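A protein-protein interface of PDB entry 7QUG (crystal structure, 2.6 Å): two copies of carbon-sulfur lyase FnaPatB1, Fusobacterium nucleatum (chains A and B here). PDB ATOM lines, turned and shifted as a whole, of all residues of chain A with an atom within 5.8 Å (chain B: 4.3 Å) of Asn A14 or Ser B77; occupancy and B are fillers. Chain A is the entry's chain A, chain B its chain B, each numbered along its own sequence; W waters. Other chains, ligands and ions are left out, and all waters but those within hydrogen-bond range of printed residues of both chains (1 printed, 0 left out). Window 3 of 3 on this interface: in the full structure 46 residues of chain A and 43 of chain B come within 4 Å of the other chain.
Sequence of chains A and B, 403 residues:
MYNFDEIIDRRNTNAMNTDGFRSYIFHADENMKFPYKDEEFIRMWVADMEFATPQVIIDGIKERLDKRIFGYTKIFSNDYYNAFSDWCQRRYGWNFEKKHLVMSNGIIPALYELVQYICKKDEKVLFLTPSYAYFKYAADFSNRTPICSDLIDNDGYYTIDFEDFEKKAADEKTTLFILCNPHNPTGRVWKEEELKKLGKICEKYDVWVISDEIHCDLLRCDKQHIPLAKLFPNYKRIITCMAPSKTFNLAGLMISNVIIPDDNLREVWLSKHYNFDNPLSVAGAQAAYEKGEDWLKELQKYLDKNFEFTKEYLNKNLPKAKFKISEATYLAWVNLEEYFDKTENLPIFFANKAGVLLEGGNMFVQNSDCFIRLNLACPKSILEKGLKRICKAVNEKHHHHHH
The side-chain amide oxygen (OD1) of Asn A14 is in hydrogen-bond range of the backbone NH (N) of Phe B76, at 2.7 Å. The side-chain amide oxygen (OD1) of Asn A14 lies within hydrogen-bond range of the backbone NH (N) of Ser B77, at 2.9 Å. The backbone carbonyl oxygen of Asn A14 lies within hydrogen-bond range of the backbone NH of Lys B74 (3.2 Å). O of Tyr B72 sits at hydrogen-bond distance from N of Met A16 (2.9 Å).
The backbone NH (N) of Asp B79 sits close to the side-chain hydroxyl (OG) of Ser B77, at 3.2 Å. O of Ala A15 lies within hydrogen-bond range of OG1 of Thr A18 (3.1 Å). The side-chain carboxylate of Asp A19 lies within hydrogen-bond range of the side-chain hydroxyl of Thr A18 (2.5 Å).
Among the printed residues, merely in contact across the chains: Asn A14 with Tyr B72, Asn A14 with Thr B73, Asn A14 with Ile B75, Ala A15 with Tyr B72, Ala A15 with Phe B76, Met A16 with Phe B76 and Asp A19 with Phe B76.
Of chain B, only Tyr B72 (3.8 Å), Thr B73 (3.3 Å), Lys B74 (3.1 Å), Ile B75 (3.6 Å), Phe B76 (2.7 Å) and Ser B77 (2.9 Å) come within 4 Å of Asn A14. Of the printed residues of chain B, Ala A15 touches Tyr B72 (3.4 Å) and Phe B76 (3.9 Å). Of the printed residues of chain A, Tyr B72 touches Asn A14, Ala A15 and Met A16. Of chain A, only Asn A14 comes within 4 Å of Ser B77. The nearest printed residue of chain B that does not touch Asn A14 is Asp B79 (6.2 Å).
Of the 8 printed residues of chain B, 6 touch a printed residue of chain A. Along chain B the printed residues that touch a printed residue of chain A span positions 72 to 77. Among the printed residues, 11 pairs touch across the chains.
No position is printed for both chains. Of the 11 pairs that touch across the chains among the printed residues, none has its exchanged pair printed and touching as well.
Water W1 lies within hydrogen-bond range of OG1 of Thr B73 and O of Thr A13.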
ATOM      1  N   ARG A  10     -17.424 -10.685  -5.463  1.00  0.00           N
ATOM      2  CA  ARG A  10     -17.284 -11.954  -4.784  1.00  0.00           C
ATOM      3  C   ARG A  10     -18.505 -12.282  -3.951  1.00  0.00           C
ATOM      4  O   ARG A  10     -18.569 -13.379  -3.385  1.00  0.00           O
ATOM      5  CB  ARG A  10     -16.042 -11.957  -3.882  1.00  0.00           C
ATOM      6  CG  ARG A  10     -14.724 -11.694  -4.579  1.00  0.00           C
ATOM      7  CD  ARG A  10     -13.564 -12.120  -3.708  1.00  0.00           C
ATOM      8  NE  ARG A  10     -13.459 -13.569  -3.502  1.00  0.00           N
ATOM      9  CZ  ARG A  10     -12.640 -14.141  -2.613  1.00  0.00           C
ATOM     10  NH1 ARG A  10     -11.866 -13.392  -1.832  1.00  0.00           N
ATOM     11  NH2 ARG A  10     -12.591 -15.461  -2.491  1.00  0.00           N
ATOM     12  N   ASN A  12     -22.029 -13.723  -3.106  1.00  0.00           N
ATOM     13  CA  ASN A  12     -22.802 -14.885  -3.562  1.00  0.00           C
ATOM     14  C   ASN A  12     -21.944 -15.911  -4.296  1.00  0.00           C
ATOM     15  O   ASN A  12     -22.329 -16.434  -5.341  1.00  0.00           O
ATOM     16  CB  ASN A  12     -23.976 -14.438  -4.415  1.00  0.00           C
ATOM     17  CG  ASN A  12     -24.843 -13.461  -3.679  1.00  0.00           C
ATOM     18  OD1 ASN A  12     -25.243 -13.730  -2.544  1.00  0.00           O
ATOM     19  ND2 ASN A  12     -25.099 -12.298  -4.284  1.00  0.00           N
ATOM     20  N   THR A  13     -20.772 -16.219  -3.718  1.00  0.00           N
ATOM     21  CA  THR A  13     -19.864 -17.226  -4.260  1.00  0.00           C
ATOM     22  C   THR A  13     -19.392 -18.199  -3.192  1.00  0.00           C
ATOM     23  O   THR A  13     -18.366 -18.861  -3.379  1.00  0.00           O
ATOM     24  CB  THR A  13     -18.649 -16.584  -4.944  1.00  0.00           C
ATOM     25  OG1 THR A  13     -17.752 -16.014  -3.969  1.00  0.00           O
ATOM     26  CG2 THR A  13     -19.110 -15.513  -5.938  1.00  0.00           C
ATOM     27  N   ASN A  14     -20.102 -18.261  -2.069  1.00  0.00           N
ATOM     28  CA  ASN A  14     -19.766 -19.120  -0.942  1.00  0.00           C
ATOM     29  C   ASN A  14     -18.310 -18.957  -0.504  1.00  0.00           C
ATOM     30  O   ASN A  14     -17.689 -19.888   0.020  1.00  0.00           O
ATOM     31  CB  ASN A  14     -20.099 -20.571  -1.270  1.00  0.00           C
ATOM     32  CG  ASN A  14     -21.570 -20.863  -1.102  1.00  0.00           C
ATOM     33  OD1 ASN A  14     -22.108 -20.790   0.006  1.00  0.00           O
ATOM     34  ND2 ASN A  14     -22.233 -21.188  -2.192  1.00  0.00           N
ATOM     35  N   ALA A  15     -17.763 -17.763  -0.709  1.00  0.00           N
ATOM     36  CA  ALA A  15     -16.410 -17.447  -0.275  1.00  0.00           C
ATOM     37  C   ALA A  15     -16.399 -17.075   1.218  1.00  0.00           C
ATOM     38  O   ALA A  15     -17.176 -16.216   1.660  1.00  0.00           O
ATOM     39  CB  ALA A  15     -15.845 -16.308  -1.137  1.00  0.00           C
ATOM     40  N   MET A  16     -15.521 -17.731   1.995  1.00  0.00           N
ATOM     41  CA  MET A  16     -15.385 -17.414   3.423  1.00  0.00           C
ATOM     42  C   MET A  16     -14.981 -15.965   3.654  1.00  0.00           C
ATOM     43  O   MET A  16     -15.376 -15.370   4.658  1.00  0.00           O
ATOM     44  CB  MET A  16     -14.348 -18.324   4.083  1.00  0.00           C
ATOM     45  CG  MET A  16     -14.178 -18.141   5.591  1.00  0.00           C
ATOM     46  SD  MET A  16     -12.808 -19.133   6.253  1.00  0.00           S
ATOM     47  CE  MET A  16     -11.465 -18.519   5.255  1.00  0.00           C
ATOM     48  N   THR A  18     -15.971 -13.252   2.271  1.00  0.00           N
ATOM     49  CA  THR A  18     -17.146 -12.391   2.368  1.00  0.00           C
ATOM     50  C   THR A  18     -18.152 -12.893   3.393  1.00  0.00           C
ATOM     51  O   THR A  18     -18.760 -12.090   4.107  1.00  0.00           O
ATOM     52  CB  THR A  18     -17.851 -12.260   1.013  1.00  0.00           C
ATOM     53  OG1 THR A  18     -18.259 -13.552   0.553  1.00  0.00           O
ATOM     54  CG2 THR A  18     -16.957 -11.598  -0.020  1.00  0.00           C
ATOM     55  N   ASP A  19     -18.310 -14.213   3.496  1.00  0.00           N
ATOM     56  CA  ASP A  19     -19.463 -14.811   4.147  1.00  0.00           C
ATOM     57  C   ASP A  19     -19.217 -15.291   5.568  1.00  0.00           C
ATOM     58  O   ASP A  19     -20.191 -15.513   6.286  1.00  0.00           O
ATOM     59  CB  ASP A  19     -19.973 -16.013   3.336  1.00  0.00           C
ATOM     60  CG  ASP A  19     -20.397 -15.648   1.921  1.00  0.00           C
ATOM     61  OD1 ASP A  19     -20.356 -14.448   1.564  1.00  0.00           O
ATOM     62  OD2 ASP A  19     -20.775 -16.578   1.166  1.00  0.00           O
ATOM     63  N   TYR B  72     -11.171 -19.629  -0.512  1.00  0.00           N
ATOM     64  CA  TYR B  72     -11.675 -20.531   0.519  1.00  0.00           C
ATOM     65  C   TYR B  72     -13.197 -20.581   0.479  1.00  0.00           C
ATOM     66  O   TYR B  72     -13.871 -19.553   0.373  1.00  0.00           O
ATOM     67  CB  TYR B  72     -11.188 -20.079   1.885  1.00  0.00           C
ATOM     68  CG  TYR B  72      -9.705 -20.262   2.071  1.00  0.00           C
ATOM     69  CD1 TYR B  72      -9.176 -21.510   2.385  1.00  0.00           C
ATOM     70  CD2 TYR B  72      -8.828 -19.181   1.935  1.00  0.00           C
ATOM     71  CE1 TYR B  72      -7.816 -21.683   2.536  1.00  0.00           C
ATOM     72  CE2 TYR B  72      -7.472 -19.343   2.091  1.00  0.00           C
ATOM     73  CZ  TYR B  72      -6.969 -20.598   2.394  1.00  0.00           C
ATOM     74  OH  TYR B  72      -5.613 -20.770   2.556  1.00  0.00           O
ATOM     75  N   THR B  73     -13.742 -21.782   0.556  1.00  0.00           N
ATOM     76  CA  THR B  73     -15.144 -21.962   0.234  1.00  0.00           C
ATOM     77  C   THR B  73     -15.776 -22.884   1.253  1.00  0.00           C
ATOM     78  O   THR B  73     -15.246 -23.964   1.540  1.00  0.00           O
ATOM     79  CB  THR B  73     -15.302 -22.517  -1.204  1.00  0.00           C
ATOM     80  OG1 THR B  73     -14.873 -21.528  -2.158  1.00  0.00           O
ATOM     81  CG2 THR B  73     -16.733 -22.938  -1.493  1.00  0.00           C
ATOM     82  N   LYS B  74     -16.887 -22.438   1.815  1.00  0.00           N
ATOM     83  CA  LYS B  74     -17.765 -23.299   2.587  1.00  0.00           C
ATOM     84  C   LYS B  74     -19.168 -23.191   2.006  1.00  0.00           C
ATOM     85  O   LYS B  74     -19.493 -22.242   1.288  1.00  0.00           O
ATOM     86  CB  LYS B  74     -17.743 -22.926   4.083  1.00  0.00           C
ATOM     87  CG  LYS B  74     -16.352 -22.999   4.712  1.00  0.00           C
ATOM     88  CD  LYS B  74     -16.379 -22.714   6.183  1.00  0.00           C
ATOM     89  CE  LYS B  74     -17.140 -23.817   6.927  1.00  0.00           C
ATOM     90  NZ  LYS B  74     -16.684 -23.935   8.340  1.00  0.00           N
ATOM     91  N   ILE B  75     -19.991 -24.197   2.269  1.00  0.00           N
ATOM     92  CA  ILE B  75     -21.358 -24.146   1.774  1.00  0.00           C
ATOM     93  C   ILE B  75     -22.151 -23.236   2.699  1.00  0.00           C
ATOM     94  O   ILE B  75     -22.744 -23.694   3.679  1.00  0.00           O
ATOM     95  CB  ILE B  75     -21.957 -25.560   1.673  1.00  0.00           C
ATOM     96  CG1 ILE B  75     -21.144 -26.360   0.637  1.00  0.00           C
ATOM     97  CG2 ILE B  75     -23.435 -25.501   1.333  1.00  0.00           C
ATOM     98  CD1 ILE B  75     -21.358 -27.851   0.663  1.00  0.00           C
ATOM     99  N   PHE B  76     -22.137 -21.933   2.397  1.00  0.00           N
ATOM    100  CA  PHE B  76     -22.759 -20.891   3.208  1.00  0.00           C
ATOM    101  C   PHE B  76     -24.224 -20.674   2.853  1.00  0.00           C
ATOM    102  O   PHE B  76     -25.054 -20.549   3.749  1.00  0.00           O
ATOM    103  CB  PHE B  76     -22.009 -19.560   3.058  1.00  0.00           C
ATOM    104  CG  PHE B  76     -20.691 -19.509   3.776  1.00  0.00           C
ATOM    105  CD1 PHE B  76     -20.645 -19.410   5.174  1.00  0.00           C
ATOM    106  CD2 PHE B  76     -19.487 -19.542   3.060  1.00  0.00           C
ATOM    107  CE1 PHE B  76     -19.417 -19.363   5.857  1.00  0.00           C
ATOM    108  CE2 PHE B  76     -18.253 -19.485   3.726  1.00  0.00           C
ATOM    109  CZ  PHE B  76     -18.220 -19.396   5.132  1.00  0.00           C
ATOM    110  N   SER B  77     -24.577 -20.627   1.573  1.00  0.00           N
ATOM    111  CA  SER B  77     -25.967 -20.341   1.259  1.00  0.00           C
ATOM    112  C   SER B  77     -26.815 -21.587   1.482  1.00  0.00           C
ATOM    113  O   SER B  77     -26.304 -22.695   1.676  1.00  0.00           O
ATOM    114  CB  SER B  77     -26.103 -19.807  -0.170  1.00  0.00           C
ATOM    115  OG  SER B  77     -26.297 -20.819  -1.122  1.00  0.00           O
ATOM    116  N   ASN B  78     -28.119 -21.384   1.565  1.00  0.00           N
ATOM    117  CA  ASN B  78     -29.002 -22.526   1.739  1.00  0.00           C
ATOM    118  C   ASN B  78     -29.360 -23.214   0.439  1.00  0.00           C
ATOM    119  O   ASN B  78     -30.141 -24.175   0.473  1.00  0.00           O
ATOM    120  CB  ASN B  78     -30.279 -22.104   2.449  1.00  0.00           C
ATOM    121  CG  ASN B  78     -30.007 -21.571   3.816  1.00  0.00           C
ATOM    122  OD1 ASN B  78     -29.186 -22.133   4.554  1.00  0.00           O
ATOM    123  ND2 ASN B  78     -30.702 -20.497   4.189  1.00  0.00           N
ATOM    124  N   ASP B  79     -28.816 -22.747  -0.688  1.00  0.00           N
ATOM    125  CA  ASP B  79     -29.189 -23.300  -1.984  1.00  0.00           C
ATOM    126  C   ASP B  79     -28.929 -24.794  -2.049  1.00  0.00           C
ATOM    127  O   ASP B  79     -29.830 -25.572  -2.379  1.00  0.00           O
ATOM    128  CB  ASP B  79     -28.441 -22.572  -3.097  1.00  0.00           C
ATOM    129  CG  ASP B  79     -28.849 -21.133  -3.192  1.00  0.00           C
ATOM    130  OD1 ASP B  79     -29.881 -20.798  -2.579  1.00  0.00           O
ATOM    131  OD2 ASP B  79     -28.152 -20.345  -3.863  1.00  0.00           O
HETATM  132  O   HOH W   1     -15.661 -19.361  -3.111  1.00  0.00           O
